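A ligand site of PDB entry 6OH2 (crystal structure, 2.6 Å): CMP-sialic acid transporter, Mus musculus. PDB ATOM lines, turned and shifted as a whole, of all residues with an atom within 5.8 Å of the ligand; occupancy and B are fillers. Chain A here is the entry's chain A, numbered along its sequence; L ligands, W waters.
The side-chain amide oxygen of Gln 101 lies close to the backbone NH of Ser 188, at 3.2 Å. OG of Ser 261 sits at hydrogen-bond distance from O of Leu 258 (2.6 Å). The side-chain amino group (NZ) of Lys 55 lies within salt-bridge range of the side-chain carboxylate (OE2) of Glu 52 (2.7 Å). The backbone carbonyl oxygen (O) of Gly 256 lies within hydrogen-bond range of the side-chain hydroxyl (OG1) of Thr 260, 2.7 Å away. The side-chain amide nitrogen of Asn 102 is in hydrogen-bond range of the backbone carbonyl oxygen of Tyr 98, 2.6 Å away. The side-chain amide nitrogen (ND2) of Asn 210 sits at hydrogen-bond distance from the side-chain hydroxyl (OG) of Ser 261, at 3.0 Å. The side-chain hydroxyl of Tyr 121 is in hydrogen-bond range of the side-chain amide nitrogen of Gln 101 (3.0 Å).
NZ of Lys 124 is in salt-bridge range of O3 of the ligand. NZ of Lys 272 is in salt-bridge range of O1 of the ligand (2.7 Å). The side-chain amide nitrogen (NE2) of Gln 101 sits at hydrogen-bond distance from an oxygen (O2) of the ligand, at 3.0 Å. O8 of the ligand sits at hydrogen-bond distance from NZ of Lys 55. OH of Tyr 121 lies within hydrogen-bond range of O3 of the ligand, at 2.7 Å. The side-chain amide oxygen of Asn 102 lies within hydrogen-bond range of an oxygen (O6) of the ligand, 2.7 Å away. The side-chain amide oxygen (OD1) of Asn 210 lies within hydrogen-bond range of a nitrogen (N3) of the ligand. A nitrogen (N2) of the ligand sits at hydrogen-bond distance from the side-chain hydroxyl (OH) of Tyr 214. The side-chain hydroxyl (OG) of Ser 188 is in hydrogen-bond range of an oxygen (O2) of the ligand (2.6 Å).
The backbone carbonyl oxygen of Gly 257 lies close to an oxygen (O8) of the ligand (3.4 Å). Merely in contact with the ligand: Tyr 98 (3.5 Å), Phe 195 (3.3 Å), Thr 260 (3.7 Å) and Ser 261 (3.3 Å). Hydrophobic or aromatic side chains within 4 Å of the ligand: Tyr 98, Tyr 121, Phe 195 and Tyr 214. 14 residues have an atom within 4 Å of the ligand: Lys 55, Tyr 98, Gln 101, Asn 102, Tyr 121, Lys 124, Ser 188, Phe 195, Asn 210, Tyr 214, Gly 257, Thr 260, Ser 261 and Lys 272. Along chain A the residues within 4 Å of the ligand span positions 55 to 272. The nearest printed residue that does not touch the ligand is Leu 258 (4.1 Å).
Water W4 lies within hydrogen-bond range of the backbone carbonyl oxygen of Ser 188, an oxygen (O2) of the ligand and the side-chain hydroxyl of Tyr 98. Water W1 lies within hydrogen-bond range of OG1 of Thr 260 (2.6 Å) and O1 of the ligand (2.9 Å). Water W3 lies within hydrogen-bond range of the side-chain amino group of Lys 55 (2.9 Å), the backbone carbonyl oxygen of Ala 253 (2.9 Å) and an oxygen (O6) of the ligand (2.9 Å). Water W2 lies within hydrogen-bond range of the side-chain hydroxyl of Tyr 121 (2.6 Å), the side-chain amide nitrogen of Gln 101 (2.7 Å) and an oxygen (O3) of the ligand (3.5 Å).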
ATOM      1  N   GLU A  52      -2.114   6.605  16.020  1.00  0.00           N
ATOM      2  CA  GLU A  52      -1.292   6.169  17.159  1.00  0.00           C
ATOM      3  C   GLU A  52      -0.260   7.225  17.564  1.00  0.00           C
ATOM      4  O   GLU A  52      -0.007   7.423  18.749  1.00  0.00           O
ATOM      5  CB  GLU A  52      -0.573   4.858  16.845  1.00  0.00           C
ATOM      6  CG  GLU A  52      -1.480   3.665  16.610  1.00  0.00           C
ATOM      7  CD  GLU A  52      -2.269   3.281  17.839  1.00  0.00           C
ATOM      8  OE1 GLU A  52      -1.649   2.962  18.868  1.00  0.00           O
ATOM      9  OE2 GLU A  52      -3.518   3.287  17.761  1.00  0.00           O
ATOM     10  N   LYS A  55      -2.243  10.072  19.387  1.00  0.00           N
ATOM     11  CA  LYS A  55      -2.607   9.552  20.710  1.00  0.00           C
ATOM     12  C   LYS A  55      -1.407   9.434  21.648  1.00  0.00           C
ATOM     13  O   LYS A  55      -1.533   9.716  22.840  1.00  0.00           O
ATOM     14  CB  LYS A  55      -3.290   8.184  20.588  1.00  0.00           C
ATOM     15  CG  LYS A  55      -4.671   8.242  19.977  1.00  0.00           C
ATOM     16  CD  LYS A  55      -5.394   6.894  20.085  1.00  0.00           C
ATOM     17  CE  LYS A  55      -4.650   5.779  19.362  1.00  0.00           C
ATOM     18  NZ  LYS A  55      -5.468   4.544  19.197  1.00  0.00           N
ATOM     19  N   TYR A  98      -5.347  -4.236  17.867  1.00  0.00           N
ATOM     20  CA  TYR A  98      -5.936  -2.949  17.485  1.00  0.00           C
ATOM     21  C   TYR A  98      -5.456  -2.447  16.127  1.00  0.00           C
ATOM     22  O   TYR A  98      -6.202  -1.749  15.440  1.00  0.00           O
ATOM     23  CB  TYR A  98      -5.703  -1.850  18.537  1.00  0.00           C
ATOM     24  CG  TYR A  98      -6.645  -1.860  19.720  1.00  0.00           C
ATOM     25  CD1 TYR A  98      -8.033  -2.023  19.549  1.00  0.00           C
ATOM     26  CD2 TYR A  98      -6.171  -1.659  21.016  1.00  0.00           C
ATOM     27  CE1 TYR A  98      -8.893  -2.024  20.642  1.00  0.00           C
ATOM     28  CE2 TYR A  98      -7.032  -1.638  22.104  1.00  0.00           C
ATOM     29  CZ  TYR A  98      -8.384  -1.820  21.915  1.00  0.00           C
ATOM     30  OH  TYR A  98      -9.240  -1.790  22.981  1.00  0.00           O
ATOM     31  N   GLN A 101      -7.844  -4.391  13.943  1.00  0.00           N
ATOM     32  CA  GLN A 101      -9.173  -3.789  14.159  1.00  0.00           C
ATOM     33  C   GLN A 101      -9.368  -2.461  13.437  1.00  0.00           C
ATOM     34  O   GLN A 101     -10.338  -2.271  12.708  1.00  0.00           O
ATOM     35  CB  GLN A 101      -9.436  -3.543  15.650  1.00  0.00           C
ATOM     36  CG  GLN A 101     -10.842  -3.016  15.972  1.00  0.00           C
ATOM     37  CD  GLN A 101     -11.039  -2.697  17.440  1.00  0.00           C
ATOM     38  OE1 GLN A 101     -10.589  -3.455  18.305  1.00  0.00           O
ATOM     39  NE2 GLN A 101     -11.696  -1.583  17.734  1.00  0.00           N
ATOM     40  N   ASN A 102      -8.451  -1.539  13.687  1.00  0.00           N
ATOM     41  CA  ASN A 102      -8.568  -0.169  13.177  1.00  0.00           C
ATOM     42  C   ASN A 102      -8.424  -0.147  11.645  1.00  0.00           C
ATOM     43  O   ASN A 102      -9.148   0.578  10.970  1.00  0.00           O
ATOM     44  CB  ASN A 102      -7.545   0.748  13.847  1.00  0.00           C
ATOM     45  CG  ASN A 102      -7.818   0.937  15.334  1.00  0.00           C
ATOM     46  OD1 ASN A 102      -8.906   1.316  15.730  1.00  0.00           O
ATOM     47  ND2 ASN A 102      -6.815   0.660  16.156  1.00  0.00           N
ATOM     48  N   TYR A 121     -21.314  -3.909  13.526  1.00  0.00           N
ATOM     49  CA  TYR A 121     -20.228  -3.760  14.486  1.00  0.00           C
ATOM     50  C   TYR A 121     -20.701  -3.854  15.963  1.00  0.00           C
ATOM     51  O   TYR A 121     -19.869  -4.088  16.850  1.00  0.00           O
ATOM     52  CB  TYR A 121     -19.448  -2.453  14.216  1.00  0.00           C
ATOM     53  CG  TYR A 121     -18.143  -2.315  15.009  1.00  0.00           C
ATOM     54  CD1 TYR A 121     -17.174  -3.312  14.974  1.00  0.00           C
ATOM     55  CD2 TYR A 121     -17.899  -1.177  15.799  1.00  0.00           C
ATOM     56  CE1 TYR A 121     -15.995  -3.197  15.706  1.00  0.00           C
ATOM     57  CE2 TYR A 121     -16.722  -1.054  16.525  1.00  0.00           C
ATOM     58  CZ  TYR A 121     -15.776  -2.056  16.474  1.00  0.00           C
ATOM     59  OH  TYR A 121     -14.602  -1.960  17.183  1.00  0.00           O
ATOM     60  N   LYS A 124     -19.786  -6.581  18.673  1.00  0.00           N
ATOM     61  CA  LYS A 124     -18.707  -6.391  19.654  1.00  0.00           C
ATOM     62  C   LYS A 124     -19.186  -6.426  21.108  1.00  0.00           C
ATOM     63  O   LYS A 124     -18.412  -6.789  21.996  1.00  0.00           O
ATOM     64  CB  LYS A 124     -17.935  -5.092  19.392  1.00  0.00           C
ATOM     65  CG  LYS A 124     -18.624  -3.815  19.834  1.00  0.00           C
ATOM     66  CD  LYS A 124     -17.720  -2.619  19.604  1.00  0.00           C
ATOM     67  CE  LYS A 124     -18.475  -1.310  19.714  1.00  0.00           C
ATOM     68  NZ  LYS A 124     -17.570  -0.143  19.933  1.00  0.00           N
ATOM     69  N   SER A 188     -12.079  -6.237  18.909  1.00  0.00           N
ATOM     70  CA  SER A 188     -12.602  -5.273  19.872  1.00  0.00           C
ATOM     71  C   SER A 188     -12.710  -5.857  21.276  1.00  0.00           C
ATOM     72  O   SER A 188     -12.228  -5.268  22.243  1.00  0.00           O
ATOM     73  CB  SER A 188     -13.968  -4.762  19.419  1.00  0.00           C
ATOM     74  OG  SER A 188     -14.444  -3.759  20.273  1.00  0.00           O
ATOM     75  N   GLY A 189     -13.358  -7.026  21.377  1.00  0.00           N
ATOM     76  CA  GLY A 189     -13.517  -7.724  22.635  1.00  0.00           C
ATOM     77  C   GLY A 189     -12.190  -8.087  23.251  1.00  0.00           C
ATOM     78  O   GLY A 189     -11.916  -7.744  24.402  1.00  0.00           O
ATOM     79  N   PHE A 195      -6.237  -4.851  27.542  1.00  0.00           N
ATOM     80  CA  PHE A 195      -5.763  -3.556  28.047  1.00  0.00           C
ATOM     81  C   PHE A 195      -6.212  -3.327  29.483  1.00  0.00           C
ATOM     82  O   PHE A 195      -5.390  -2.990  30.340  1.00  0.00           O
ATOM     83  CB  PHE A 195      -6.239  -2.397  27.153  1.00  0.00           C
ATOM     84  CG  PHE A 195      -5.837  -1.047  27.665  1.00  0.00           C
ATOM     85  CD1 PHE A 195      -4.556  -0.561  27.441  1.00  0.00           C
ATOM     86  CD2 PHE A 195      -6.716  -0.285  28.436  1.00  0.00           C
ATOM     87  CE1 PHE A 195      -4.164   0.670  27.937  1.00  0.00           C
ATOM     88  CE2 PHE A 195      -6.335   0.946  28.934  1.00  0.00           C
ATOM     89  CZ  PHE A 195      -5.058   1.427  28.689  1.00  0.00           C
ATOM     90  N   ASN A 210      -1.228   3.775  28.272  1.00  0.00           N
ATOM     91  CA  ASN A 210      -1.436   4.262  26.910  1.00  0.00           C
ATOM     92  C   ASN A 210      -0.121   4.499  26.172  1.00  0.00           C
ATOM     93  O   ASN A 210       0.006   4.079  25.017  1.00  0.00           O
ATOM     94  CB  ASN A 210      -2.303   5.538  26.926  1.00  0.00           C
ATOM     95  CG  ASN A 210      -3.776   5.238  27.139  1.00  0.00           C
ATOM     96  OD1 ASN A 210      -4.198   4.083  27.102  1.00  0.00           O
ATOM     97  ND2 ASN A 210      -4.572   6.288  27.358  1.00  0.00           N
ATOM     98  N   MET A 213       1.604   1.276  25.305  1.00  0.00           N
ATOM     99  CA  MET A 213       0.862   0.633  24.225  1.00  0.00           C
ATOM    100  C   MET A 213       1.075   1.318  22.887  1.00  0.00           C
ATOM    101  O   MET A 213       1.435   0.653  21.917  1.00  0.00           O
ATOM    102  CB  MET A 213      -0.635   0.607  24.543  1.00  0.00           C
ATOM    103  CG  MET A 213      -1.425  -0.419  23.758  1.00  0.00           C
ATOM    104  SD  MET A 213      -3.189  -0.049  23.797  1.00  0.00           S
ATOM    105  CE  MET A 213      -3.831  -1.695  23.915  1.00  0.00           C
ATOM    106  N   TYR A 214       0.856   2.638  22.825  1.00  0.00           N
ATOM    107  CA  TYR A 214       0.930   3.373  21.553  1.00  0.00           C
ATOM    108  C   TYR A 214       2.332   3.390  20.956  1.00  0.00           C
ATOM    109  O   TYR A 214       2.474   3.579  19.747  1.00  0.00           O
ATOM    110  CB  TYR A 214       0.410   4.817  21.673  1.00  0.00           C
ATOM    111  CG  TYR A 214      -1.009   4.975  22.217  1.00  0.00           C
ATOM    112  CD1 TYR A 214      -2.024   4.081  21.897  1.00  0.00           C
ATOM    113  CD2 TYR A 214      -1.327   6.044  23.050  1.00  0.00           C
ATOM    114  CE1 TYR A 214      -3.308   4.221  22.401  1.00  0.00           C
ATOM    115  CE2 TYR A 214      -2.600   6.206  23.561  1.00  0.00           C
ATOM    116  CZ  TYR A 214      -3.585   5.291  23.239  1.00  0.00           C
ATOM    117  OH  TYR A 214      -4.854   5.465  23.765  1.00  0.00           O
ATOM    118  N   ALA A 253     -10.519   9.669  15.502  1.00  0.00           N
ATOM    119  CA  ALA A 253     -10.010   8.356  15.936  1.00  0.00           C
ATOM    120  C   ALA A 253      -9.100   8.459  17.158  1.00  0.00           C
ATOM    121  O   ALA A 253      -9.138   7.593  18.030  1.00  0.00           O
ATOM    122  CB  ALA A 253      -9.268   7.672  14.796  1.00  0.00           C
ATOM    123  N   SER A 254      -8.288   9.516  17.184  1.00  0.00           N
ATOM    124  CA  SER A 254      -7.336   9.752  18.285  1.00  0.00           C
ATOM    125  C   SER A 254      -8.055  10.086  19.583  1.00  0.00           C
ATOM    126  O   SER A 254      -7.770   9.501  20.641  1.00  0.00           O
ATOM    127  CB  SER A 254      -6.369  10.890  17.919  1.00  0.00           C
ATOM    128  OG  SER A 254      -5.598  10.577  16.765  1.00  0.00           O
ATOM    129  N   GLY A 256     -11.364   9.613  20.229  1.00  0.00           N
ATOM    130  CA  GLY A 256     -12.164   8.443  20.561  1.00  0.00           C
ATOM    131  C   GLY A 256     -11.366   7.316  21.202  1.00  0.00           C
ATOM    132  O   GLY A 256     -11.851   6.651  22.116  1.00  0.00           O
ATOM    133  N   GLY A 257     -10.147   7.102  20.720  1.00  0.00           N
ATOM    134  CA  GLY A 257      -9.255   6.096  21.293  1.00  0.00           C
ATOM    135  C   GLY A 257      -8.875   6.419  22.731  1.00  0.00           C
ATOM    136  O   GLY A 257      -8.982   5.579  23.621  1.00  0.00           O
ATOM    137  N   LEU A 258      -8.435   7.656  22.946  1.00  0.00           N
ATOM    138  CA  LEU A 258      -8.043   8.124  24.272  1.00  0.00           C
ATOM    139  C   LEU A 258      -9.226   8.092  25.246  1.00  0.00           C
ATOM    140  O   LEU A 258      -9.092   7.627  26.380  1.00  0.00           O
ATOM    141  CB  LEU A 258      -7.447   9.539  24.199  1.00  0.00           C
ATOM    142  CG  LEU A 258      -6.116   9.708  23.437  1.00  0.00           C
ATOM    143  CD1 LEU A 258      -5.877  11.152  23.056  1.00  0.00           C
ATOM    144  CD2 LEU A 258      -4.948   9.170  24.233  1.00  0.00           C
ATOM    145  N   THR A 260     -11.981   6.280  24.988  1.00  0.00           N
ATOM    146  CA  THR A 260     -12.298   4.868  25.252  1.00  0.00           C
ATOM    147  C   THR A 260     -11.491   4.334  26.450  1.00  0.00           C
ATOM    148  O   THR A 260     -12.043   3.619  27.287  1.00  0.00           O
ATOM    149  CB  THR A 260     -12.024   3.959  24.015  1.00  0.00           C
ATOM    150  OG1 THR A 260     -12.892   4.332  22.938  1.00  0.00           O
ATOM    151  CG2 THR A 260     -12.254   2.485  24.340  1.00  0.00           C
ATOM    152  N   SER A 261     -10.200   4.698  26.525  1.00  0.00           N
ATOM    153  CA  SER A 261      -9.327   4.231  27.613  1.00  0.00           C
ATOM    154  C   SER A 261      -9.746   4.779  28.987  1.00  0.00           C
ATOM    155  O   SER A 261      -9.646   4.071  29.988  1.00  0.00           O
ATOM    156  CB  SER A 261      -7.849   4.559  27.336  1.00  0.00           C
ATOM    157  OG  SER A 261      -7.542   5.922  27.565  1.00  0.00           O
ATOM    158  N   LYS A 272     -18.711   0.166  29.092  1.00  0.00           N
ATOM    159  CA  LYS A 272     -18.451   0.959  27.878  1.00  0.00           C
ATOM    160  C   LYS A 272     -19.622   0.856  26.868  1.00  0.00           C
ATOM    161  O   LYS A 272     -20.004   1.865  26.281  1.00  0.00           O
ATOM    162  CB  LYS A 272     -17.143   0.492  27.220  1.00  0.00           C
ATOM    163  CG  LYS A 272     -16.662   1.332  26.040  1.00  0.00           C
ATOM    164  CD  LYS A 272     -15.456   0.703  25.367  1.00  0.00           C
ATOM    165  CE  LYS A 272     -15.832  -0.451  24.446  1.00  0.00           C
ATOM    166  NZ  LYS A 272     -14.656  -1.178  23.902  1.00  0.00           N
HETATM  167  O1  LIG L   1     -14.397   0.308  21.626  1.00  0.00           O
HETATM  168  P1  LIG L   1     -13.894  -0.231  20.307  1.00  0.00           P
HETATM  169  O2  LIG L   1     -13.098  -1.525  20.334  1.00  0.00           O
HETATM  170  O3  LIG L   1     -14.916  -0.188  19.197  1.00  0.00           O
HETATM  171  O4  LIG L   1     -12.827   0.878  19.879  1.00  0.00           O
HETATM  172  C1  LIG L   1     -11.619   0.966  20.601  1.00  0.00           C
HETATM  173  C2  LIG L   1     -10.808   2.092  20.000  1.00  0.00           C
HETATM  174  O5  LIG L   1     -10.098   2.706  21.070  1.00  0.00           O
HETATM  175  C3  LIG L   1      -9.771   1.622  19.003  1.00  0.00           C
HETATM  176  O6  LIG L   1      -9.683   2.605  17.956  1.00  0.00           O
HETATM  177  C4  LIG L   1      -8.481   1.553  19.801  1.00  0.00           C
HETATM  178  O7  LIG L   1      -7.324   1.803  19.006  1.00  0.00           O
HETATM  179  C5  LIG L   1      -8.691   2.664  20.802  1.00  0.00           C
HETATM  180  N1  LIG L   1      -7.996   2.526  22.087  1.00  0.00           N
HETATM  181  C6  LIG L   1      -6.920   3.399  22.399  1.00  0.00           C
HETATM  182  N2  LIG L   1      -6.300   3.299  23.587  1.00  0.00           N
HETATM  183  C7  LIG L   1      -6.679   2.372  24.488  1.00  0.00           C
HETATM  184  C8  LIG L   1      -7.737   1.517  24.210  1.00  0.00           C
HETATM  185  C9  LIG L   1      -8.396   1.606  22.986  1.00  0.00           C
HETATM  186  O8  LIG L   1      -6.527   4.266  21.598  1.00  0.00           O
HETATM  187  N3  LIG L   1      -6.021   2.309  25.665  1.00  0.00           N
HETATM  188  O   HOH W   1     -15.097   2.916  22.563  1.00  0.00           O
HETATM  189  O   HOH W   2     -13.263  -0.038  16.144  1.00  0.00           O
HETATM  190  O   HOH W   3      -7.952   4.964  17.832  1.00  0.00           O
HETATM  191  O   HOH W   4     -11.743  -2.666  22.303  1.00  0.00           O
